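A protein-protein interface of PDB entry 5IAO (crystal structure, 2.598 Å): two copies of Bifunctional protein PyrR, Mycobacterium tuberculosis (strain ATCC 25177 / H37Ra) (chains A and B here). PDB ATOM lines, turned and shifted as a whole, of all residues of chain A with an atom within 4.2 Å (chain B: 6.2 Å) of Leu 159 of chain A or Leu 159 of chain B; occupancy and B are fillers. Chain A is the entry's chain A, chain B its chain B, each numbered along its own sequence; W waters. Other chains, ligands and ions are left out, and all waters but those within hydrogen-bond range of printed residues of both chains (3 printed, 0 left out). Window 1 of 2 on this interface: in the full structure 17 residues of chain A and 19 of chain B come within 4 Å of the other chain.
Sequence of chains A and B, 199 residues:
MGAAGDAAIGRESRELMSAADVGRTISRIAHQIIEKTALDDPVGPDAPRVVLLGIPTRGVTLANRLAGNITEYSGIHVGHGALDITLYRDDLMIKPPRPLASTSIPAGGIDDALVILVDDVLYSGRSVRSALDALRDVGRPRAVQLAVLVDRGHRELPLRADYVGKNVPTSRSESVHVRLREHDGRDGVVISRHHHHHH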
ATOM      1  N   GLY A 125      16.635  -5.720 -14.400  1.00  0.00           N
ATOM      2  CA  GLY A 125      17.685  -5.714 -15.399  1.00  0.00           C
ATOM      3  C   GLY A 125      19.052  -5.917 -14.777  1.00  0.00           C
ATOM      4  O   GLY A 125      20.068  -5.992 -15.483  1.00  0.00           O
ATOM      5  N   VAL A 128      21.042  -9.217 -15.769  1.00  0.00           N
ATOM      6  CA  VAL A 128      21.603  -9.092 -17.105  1.00  0.00           C
ATOM      7  C   VAL A 128      22.856  -8.216 -17.107  1.00  0.00           C
ATOM      8  O   VAL A 128      23.834  -8.529 -17.786  1.00  0.00           O
ATOM      9  CB  VAL A 128      20.559  -8.527 -18.085  1.00  0.00           C
ATOM     10  CG1 VAL A 128      21.228  -7.924 -19.318  1.00  0.00           C
ATOM     11  CG2 VAL A 128      19.545  -9.613 -18.449  1.00  0.00           C
ATOM     12  N   ARG A 129      22.841  -7.133 -16.332  1.00  0.00           N
ATOM     13  CA  ARG A 129      24.018  -6.270 -16.238  1.00  0.00           C
ATOM     14  C   ARG A 129      25.190  -7.056 -15.644  1.00  0.00           C
ATOM     15  O   ARG A 129      26.329  -6.914 -16.092  1.00  0.00           O
ATOM     16  CB  ARG A 129      23.726  -5.027 -15.397  1.00  0.00           C
ATOM     17  CG  ARG A 129      24.933  -4.128 -15.192  1.00  0.00           C
ATOM     18  CD  ARG A 129      25.205  -3.881 -13.726  1.00  0.00           C
ATOM     19  NE  ARG A 129      25.391  -2.461 -13.432  1.00  0.00           N
ATOM     20  CZ  ARG A 129      26.418  -1.741 -13.869  1.00  0.00           C
ATOM     21  NH1 ARG A 129      27.344  -2.305 -14.634  1.00  0.00           N
ATOM     22  NH2 ARG A 129      26.510  -0.457 -13.551  1.00  0.00           N
ATOM     23  N   LEU A 132      26.647  -9.066 -18.290  1.00  0.00           N
ATOM     24  CA  LEU A 132      27.507  -8.235 -19.130  1.00  0.00           C
ATOM     25  C   LEU A 132      28.893  -8.093 -18.512  1.00  0.00           C
ATOM     26  O   LEU A 132      29.898  -8.195 -19.212  1.00  0.00           O
ATOM     27  CB  LEU A 132      26.884  -6.848 -19.356  1.00  0.00           C
ATOM     28  CG  LEU A 132      25.621  -6.814 -20.229  1.00  0.00           C
ATOM     29  CD1 LEU A 132      25.058  -5.412 -20.336  1.00  0.00           C
ATOM     30  CD2 LEU A 132      25.902  -7.367 -21.622  1.00  0.00           C
ATOM     31  N   ARG A 155      12.066  -1.972 -15.110  1.00  0.00           N
ATOM     32  CA  ARG A 155      13.511  -2.013 -15.264  1.00  0.00           C
ATOM     33  C   ARG A 155      14.131  -0.900 -14.418  1.00  0.00           C
ATOM     34  O   ARG A 155      13.515   0.141 -14.205  1.00  0.00           O
ATOM     35  CB  ARG A 155      13.915  -1.880 -16.737  1.00  0.00           C
ATOM     36  CG  ARG A 155      13.619  -0.532 -17.349  1.00  0.00           C
ATOM     37  CD  ARG A 155      13.980  -0.499 -18.824  1.00  0.00           C
ATOM     38  NE  ARG A 155      13.557   0.751 -19.456  1.00  0.00           N
ATOM     39  CZ  ARG A 155      12.358   0.956 -19.995  1.00  0.00           C
ATOM     40  NH1 ARG A 155      11.449  -0.009 -19.977  1.00  0.00           N
ATOM     41  NH2 ARG A 155      12.064   2.130 -20.546  1.00  0.00           N
ATOM     42  N   LEU A 157      17.479  -0.201 -15.068  1.00  0.00           N
ATOM     43  CA  LEU A 157      18.612   0.132 -15.924  1.00  0.00           C
ATOM     44  C   LEU A 157      18.118   0.266 -17.360  1.00  0.00           C
ATOM     45  O   LEU A 157      17.083  -0.298 -17.712  1.00  0.00           O
ATOM     46  CB  LEU A 157      19.707  -0.943 -15.834  1.00  0.00           C
ATOM     47  CG  LEU A 157      20.389  -1.171 -14.481  1.00  0.00           C
ATOM     48  CD1 LEU A 157      21.204  -2.450 -14.490  1.00  0.00           C
ATOM     49  CD2 LEU A 157      21.274   0.010 -14.121  1.00  0.00           C
ATOM     50  N   PRO A 158      18.851   1.019 -18.195  1.00  0.00           N
ATOM     51  CA  PRO A 158      18.461   1.190 -19.600  1.00  0.00           C
ATOM     52  C   PRO A 158      18.763  -0.065 -20.429  1.00  0.00           C
ATOM     53  O   PRO A 158      19.390   0.007 -21.485  1.00  0.00           O
ATOM     54  CB  PRO A 158      19.307   2.379 -20.055  1.00  0.00           C
ATOM     55  CG  PRO A 158      20.522   2.315 -19.192  1.00  0.00           C
ATOM     56  CD  PRO A 158      20.070   1.776 -17.859  1.00  0.00           C
ATOM     57  N   LEU A 159      18.326  -1.212 -19.921  1.00  0.00           N
ATOM     58  CA  LEU A 159      18.486  -2.488 -20.606  1.00  0.00           C
ATOM     59  C   LEU A 159      17.166  -3.021 -21.151  1.00  0.00           C
ATOM     60  O   LEU A 159      16.162  -3.052 -20.442  1.00  0.00           O
ATOM     61  CB  LEU A 159      19.095  -3.530 -19.668  1.00  0.00           C
ATOM     62  CG  LEU A 159      20.523  -3.298 -19.189  1.00  0.00           C
ATOM     63  CD1 LEU A 159      20.856  -4.275 -18.082  1.00  0.00           C
ATOM     64  CD2 LEU A 159      21.500  -3.450 -20.348  1.00  0.00           C
ATOM     65  N   ARG A 160      17.183  -3.470 -22.400  1.00  0.00           N
ATOM     66  CA  ARG A 160      16.004  -4.057 -23.020  1.00  0.00           C
ATOM     67  C   ARG A 160      16.382  -5.366 -23.707  1.00  0.00           C
ATOM     68  O   ARG A 160      17.510  -5.514 -24.188  1.00  0.00           O
ATOM     69  CB  ARG A 160      15.384  -3.096 -24.038  1.00  0.00           C
ATOM     70  CG  ARG A 160      15.151  -1.681 -23.518  1.00  0.00           C
ATOM     71  CD  ARG A 160      14.274  -1.686 -22.279  1.00  0.00           C
ATOM     72  NE  ARG A 160      12.887  -2.030 -22.575  1.00  0.00           N
ATOM     73  CZ  ARG A 160      12.094  -2.711 -21.749  1.00  0.00           C
ATOM     74  NH1 ARG A 160      12.556  -3.132 -20.572  1.00  0.00           N
ATOM     75  NH2 ARG A 160      10.839  -2.976 -22.101  1.00  0.00           N
ATOM     76  N   LEU B 122      23.285   7.966 -29.450  1.00  0.00           N
ATOM     77  CA  LEU B 122      23.386   6.569 -29.054  1.00  0.00           C
ATOM     78  C   LEU B 122      23.787   5.750 -30.277  1.00  0.00           C
ATOM     79  O   LEU B 122      23.117   5.798 -31.311  1.00  0.00           O
ATOM     80  CB  LEU B 122      22.068   6.067 -28.463  1.00  0.00           C
ATOM     81  CG  LEU B 122      22.080   4.619 -27.970  1.00  0.00           C
ATOM     82  CD1 LEU B 122      23.202   4.412 -26.971  1.00  0.00           C
ATOM     83  CD2 LEU B 122      20.752   4.251 -27.349  1.00  0.00           C
ATOM     84  N   SER B 124      26.783   2.365 -30.603  1.00  0.00           N
ATOM     85  CA  SER B 124      27.028   0.995 -30.167  1.00  0.00           C
ATOM     86  C   SER B 124      26.524   0.782 -28.738  1.00  0.00           C
ATOM     87  O   SER B 124      26.180  -0.337 -28.343  1.00  0.00           O
ATOM     88  CB  SER B 124      28.520   0.661 -30.241  1.00  0.00           C
ATOM     89  OG  SER B 124      29.223   1.231 -29.146  1.00  0.00           O
ATOM     90  N   GLY B 125      26.519   1.861 -27.959  1.00  0.00           N
ATOM     91  CA  GLY B 125      26.071   1.807 -26.581  1.00  0.00           C
ATOM     92  C   GLY B 125      27.189   1.647 -25.566  1.00  0.00           C
ATOM     93  O   GLY B 125      26.937   1.572 -24.362  1.00  0.00           O
ATOM     94  N   ARG B 126      28.426   1.574 -26.043  1.00  0.00           N
ATOM     95  CA  ARG B 126      29.553   1.313 -25.151  1.00  0.00           C
ATOM     96  C   ARG B 126      29.846   2.505 -24.242  1.00  0.00           C
ATOM     97  O   ARG B 126      30.246   2.327 -23.091  1.00  0.00           O
ATOM     98  CB  ARG B 126      30.792   0.937 -25.962  1.00  0.00           C
ATOM     99  CG  ARG B 126      30.613  -0.366 -26.712  1.00  0.00           C
ATOM    100  CD  ARG B 126      31.900  -0.878 -27.315  1.00  0.00           C
ATOM    101  NE  ARG B 126      31.672  -2.107 -28.077  1.00  0.00           N
ATOM    102  CZ  ARG B 126      31.438  -3.301 -27.533  1.00  0.00           C
ATOM    103  NH1 ARG B 126      31.386  -3.438 -26.211  1.00  0.00           N
ATOM    104  NH2 ARG B 126      31.244  -4.361 -28.311  1.00  0.00           N
ATOM    105  N   VAL B 128      27.570   4.503 -23.054  1.00  0.00           N
ATOM    106  CA  VAL B 128      26.569   4.431 -22.006  1.00  0.00           C
ATOM    107  C   VAL B 128      26.932   3.367 -20.973  1.00  0.00           C
ATOM    108  O   VAL B 128      26.826   3.604 -19.767  1.00  0.00           O
ATOM    109  CB  VAL B 128      25.170   4.147 -22.590  1.00  0.00           C
ATOM    110  CG1 VAL B 128      24.212   3.635 -21.512  1.00  0.00           C
ATOM    111  CG2 VAL B 128      24.623   5.406 -23.265  1.00  0.00           C
ATOM    112  N   ARG B 129      27.425   2.220 -21.433  1.00  0.00           N
ATOM    113  CA  ARG B 129      27.799   1.156 -20.505  1.00  0.00           C
ATOM    114  C   ARG B 129      28.942   1.622 -19.597  1.00  0.00           C
ATOM    115  O   ARG B 129      28.981   1.300 -18.409  1.00  0.00           O
ATOM    116  CB  ARG B 129      28.197  -0.118 -21.242  1.00  0.00           C
ATOM    117  CG  ARG B 129      28.560  -1.229 -20.273  1.00  0.00           C
ATOM    118  CD  ARG B 129      29.942  -1.816 -20.434  1.00  0.00           C
ATOM    119  NE  ARG B 129      30.044  -3.002 -19.589  1.00  0.00           N
ATOM    120  CZ  ARG B 129      30.086  -4.248 -20.046  1.00  0.00           C
ATOM    121  NH1 ARG B 129      30.067  -4.477 -21.353  1.00  0.00           N
ATOM    122  NH2 ARG B 129      30.164  -5.264 -19.193  1.00  0.00           N
ATOM    123  N   LEU B 132      27.430   3.570 -16.934  1.00  0.00           N
ATOM    124  CA  LEU B 132      26.875   2.708 -15.902  1.00  0.00           C
ATOM    125  C   LEU B 132      27.975   2.265 -14.928  1.00  0.00           C
ATOM    126  O   LEU B 132      27.754   2.201 -13.721  1.00  0.00           O
ATOM    127  CB  LEU B 132      26.187   1.492 -16.527  1.00  0.00           C
ATOM    128  CG  LEU B 132      24.927   1.745 -17.362  1.00  0.00           C
ATOM    129  CD1 LEU B 132      24.385   0.424 -17.923  1.00  0.00           C
ATOM    130  CD2 LEU B 132      23.853   2.516 -16.584  1.00  0.00           C
ATOM    131  N   VAL B 144      18.161   3.844 -13.185  1.00  0.00           N
ATOM    132  CA  VAL B 144      18.898   4.617 -14.180  1.00  0.00           C
ATOM    133  C   VAL B 144      18.156   4.607 -15.502  1.00  0.00           C
ATOM    134  O   VAL B 144      17.840   3.547 -16.032  1.00  0.00           O
ATOM    135  CB  VAL B 144      20.326   4.074 -14.413  1.00  0.00           C
ATOM    136  CG1 VAL B 144      21.077   4.957 -15.402  1.00  0.00           C
ATOM    137  CG2 VAL B 144      21.082   3.949 -13.097  1.00  0.00           C
ATOM    138  N   LEU B 146      17.953   6.607 -19.573  1.00  0.00           N
ATOM    139  CA  LEU B 146      18.835   7.178 -20.573  1.00  0.00           C
ATOM    140  C   LEU B 146      18.045   8.049 -21.545  1.00  0.00           C
ATOM    141  O   LEU B 146      17.016   7.624 -22.073  1.00  0.00           O
ATOM    142  CB  LEU B 146      19.572   6.063 -21.324  1.00  0.00           C
ATOM    143  CG  LEU B 146      20.402   6.472 -22.541  1.00  0.00           C
ATOM    144  CD1 LEU B 146      21.517   7.399 -22.111  1.00  0.00           C
ATOM    145  CD2 LEU B 146      20.970   5.253 -23.263  1.00  0.00           C
ATOM    146  N   ARG B 155      23.460  -0.934 -32.239  1.00  0.00           N
ATOM    147  CA  ARG B 155      23.869  -1.227 -30.871  1.00  0.00           C
ATOM    148  C   ARG B 155      24.648  -2.533 -30.829  1.00  0.00           C
ATOM    149  O   ARG B 155      24.397  -3.441 -31.621  1.00  0.00           O
ATOM    150  CB  ARG B 155      22.665  -1.299 -29.933  1.00  0.00           C
ATOM    151  CG  ARG B 155      21.723  -2.451 -30.203  1.00  0.00           C
ATOM    152  CD  ARG B 155      20.551  -2.403 -29.232  1.00  0.00           C
ATOM    153  NE  ARG B 155      19.513  -3.382 -29.540  1.00  0.00           N
ATOM    154  CZ  ARG B 155      18.498  -3.150 -30.366  1.00  0.00           C
ATOM    155  NH1 ARG B 155      18.399  -1.975 -30.977  1.00  0.00           N
ATOM    156  NH2 ARG B 155      17.586  -4.090 -30.589  1.00  0.00           N
ATOM    157  N   LEU B 157      25.211  -3.763 -27.631  1.00  0.00           N
ATOM    158  CA  LEU B 157      24.803  -4.199 -26.302  1.00  0.00           C
ATOM    159  C   LEU B 157      23.296  -4.037 -26.173  1.00  0.00           C
ATOM    160  O   LEU B 157      22.701  -3.225 -26.881  1.00  0.00           O
ATOM    161  CB  LEU B 157      25.531  -3.395 -25.233  1.00  0.00           C
ATOM    162  CG  LEU B 157      27.051  -3.549 -25.220  1.00  0.00           C
ATOM    163  CD1 LEU B 157      27.678  -2.482 -24.342  1.00  0.00           C
ATOM    164  CD2 LEU B 157      27.441  -4.940 -24.729  1.00  0.00           C
ATOM    165  N   PRO B 158      22.665  -4.808 -25.274  1.00  0.00           N
ATOM    166  CA  PRO B 158      21.212  -4.706 -25.085  1.00  0.00           C
ATOM    167  C   PRO B 158      20.810  -3.448 -24.310  1.00  0.00           C
ATOM    168  O   PRO B 158      20.038  -3.527 -23.354  1.00  0.00           O
ATOM    169  CB  PRO B 158      20.874  -5.969 -24.289  1.00  0.00           C
ATOM    170  CG  PRO B 158      22.123  -6.269 -23.528  1.00  0.00           C
ATOM    171  CD  PRO B 158      23.270  -5.836 -24.409  1.00  0.00           C
ATOM    172  N   LEU B 159      21.337  -2.299 -24.727  1.00  0.00           N
ATOM    173  CA  LEU B 159      21.004  -1.028 -24.102  1.00  0.00           C
ATOM    174  C   LEU B 159      20.104  -0.206 -25.007  1.00  0.00           C
ATOM    175  O   LEU B 159      20.380  -0.069 -26.192  1.00  0.00           O
ATOM    176  CB  LEU B 159      22.265  -0.227 -23.786  1.00  0.00           C
ATOM    177  CG  LEU B 159      23.238  -0.776 -22.752  1.00  0.00           C
ATOM    178  CD1 LEU B 159      24.514   0.039 -22.775  1.00  0.00           C
ATOM    179  CD2 LEU B 159      22.615  -0.765 -21.368  1.00  0.00           C
ATOM    180  N   ARG B 160      19.033   0.347 -24.447  1.00  0.00           N
ATOM    181  CA  ARG B 160      18.137   1.202 -25.210  1.00  0.00           C
ATOM    182  C   ARG B 160      17.832   2.466 -24.411  1.00  0.00           C
ATOM    183  O   ARG B 160      17.834   2.447 -23.181  1.00  0.00           O
ATOM    184  CB  ARG B 160      16.840   0.472 -25.579  1.00  0.00           C
ATOM    185  CG  ARG B 160      17.047  -0.902 -26.212  1.00  0.00           C
ATOM    186  CD  ARG B 160      17.966  -0.817 -27.425  1.00  0.00           C
ATOM    187  NE  ARG B 160      17.378  -0.145 -28.579  1.00  0.00           N
ATOM    188  CZ  ARG B 160      18.072   0.613 -29.428  1.00  0.00           C
ATOM    189  NH1 ARG B 160      19.374   0.810 -29.234  1.00  0.00           N
ATOM    190  NH2 ARG B 160      17.466   1.188 -30.461  1.00  0.00           N
ATOM    191  N   ALA B 161      17.603   3.565 -25.123  1.00  0.00           N
ATOM    192  CA  ALA B 161      17.252   4.835 -24.502  1.00  0.00           C
ATOM    193  C   ALA B 161      15.797   4.861 -24.064  1.00  0.00           C
ATOM    194  O   ALA B 161      14.935   4.316 -24.738  1.00  0.00           O
ATOM    195  CB  ALA B 161      17.532   5.982 -25.460  1.00  0.00           C
HETATM  196  O   HOH W   1      28.804  -3.015 -16.473  1.00  0.00           O
HETATM  197  O   HOH W   2      25.101   1.626 -12.705  1.00  0.00           O
HETATM  198  O   HOH W   3      15.453   1.522 -21.833  1.00  0.00           O
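Water W1 lies within hydrogen-bond range of the guanidinium group (NH1) of Arg 129 of chain A (2.5 Å) and the guanidinium group (NE) of Arg 129 of chain B (3.4 Å).
Water W2 bridges the guanidinium group (NH2) of Arg 129 of chain A (2.7 Å) and the backbone carbonyl oxygen (O) of Leu 132 of chain B (2.9 Å).
Water W3 bridges the backbone carbonyl oxygen (O) of Arg 160 of chain B (2.9 Å) and the guanidinium group (NE) of Arg 155 of chain A (3.1 Å).
Among the printed residues, merely in contact across the chains: Leu 159 of chain A with Leu 159 of chain B (3.1 Å), Pro 158 of chain A with Leu 159 of chain B (3.2 Å), Leu 159 of chain A with Pro 158 of chain B (3.3 Å), Arg 160 of chain A with Arg 160 of chain B (3.4 Å), Leu 157 of chain A with Val 144 of chain B (3.5 Å) and Pro 158 of chain A with Leu 146 of chain B (3.9 Å).
Of the 9 printed residues of chain A, 6 touch a printed residue of chain B.
Of the 15 printed residues of chain B, 7 touch a printed residue of chain A.
Printed residues of chain B that touch a printed residue of chain A: Arg 129, Leu 132, Val 144, Leu 146, Pro 158, Leu 159 and Arg 160.
Hydrophobic or aromatic side chains of chain B within 4 Å of the printed part of chain A: Leu 132, Leu 146, Pro 158 and Leu 159.
Among the printed residues, no Asp or Glu carboxylate lies within 4 Å of a Lys or Arg side-chain nitrogen of the other chain.
The backbone carbonyl oxygen of Leu 132 of chain B is in hydrogen-bond range of the guanidinium group of Arg 129 of chain A.
O of Leu 132 of chain A lies within hydrogen-bond range of NH2 of Arg 129 of chain B, 2.9 Å away.
The backbone carbonyl oxygen of Pro 158 of chain A is in hydrogen-bond range of the backbone NH of Arg 160 of chain B.
The backbone NH of Arg 160 of chain A sits at hydrogen-bond distance from the backbone carbonyl oxygen of Pro 158 of chain B, at 3.0 Å.
The backbone nitrogen (N) of Pro 158 of chain A sits close to the backbone carbonyl oxygen (O) of Val 144 of chain B, 3.5 Å away.
Arg 129 of chain A touches Leu 132 of chain B, and with the chains exchanged Leu 132 of chain A touches Arg 129 of chain B.
Pro 158 of chain A touches Leu 159 of chain B, and with the chains exchanged Leu 159 of chain A touches Pro 158 of chain B.
Leu 159 of chain A touches its own counterpart, Leu 159 of chain B.
Arg 160 of chain A touches its own counterpart, Arg 160 of chain B.
Leu 159 of chain A touches just these residues of chain B: Pro 158 (3.3 Å) and Leu 159 (3.1 Å).
Of the printed residues of chain B, Arg 160 of chain A touches Pro 158 (3.0 Å) and Arg 160 (3.4 Å).
Arg 126 of chain B touches none of the printed residues of chain A.
Val 128 of chain B touches none of the printed residues of chain A.
Printed residues of chain A within 4 Å of Arg 129 of chain B: Leu 132.
Of chain A, only Pro 158 and Leu 159 come within 4 Å of Leu 159 of chain B.
The nearest residue of chain B that does not touch Leu 159 of chain A is Arg 160 of chain B (4.8 Å).
The nearest printed residue of chain A that does not touch Pro 158 of chain B is Pro 158 of chain A (4.05 Å).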
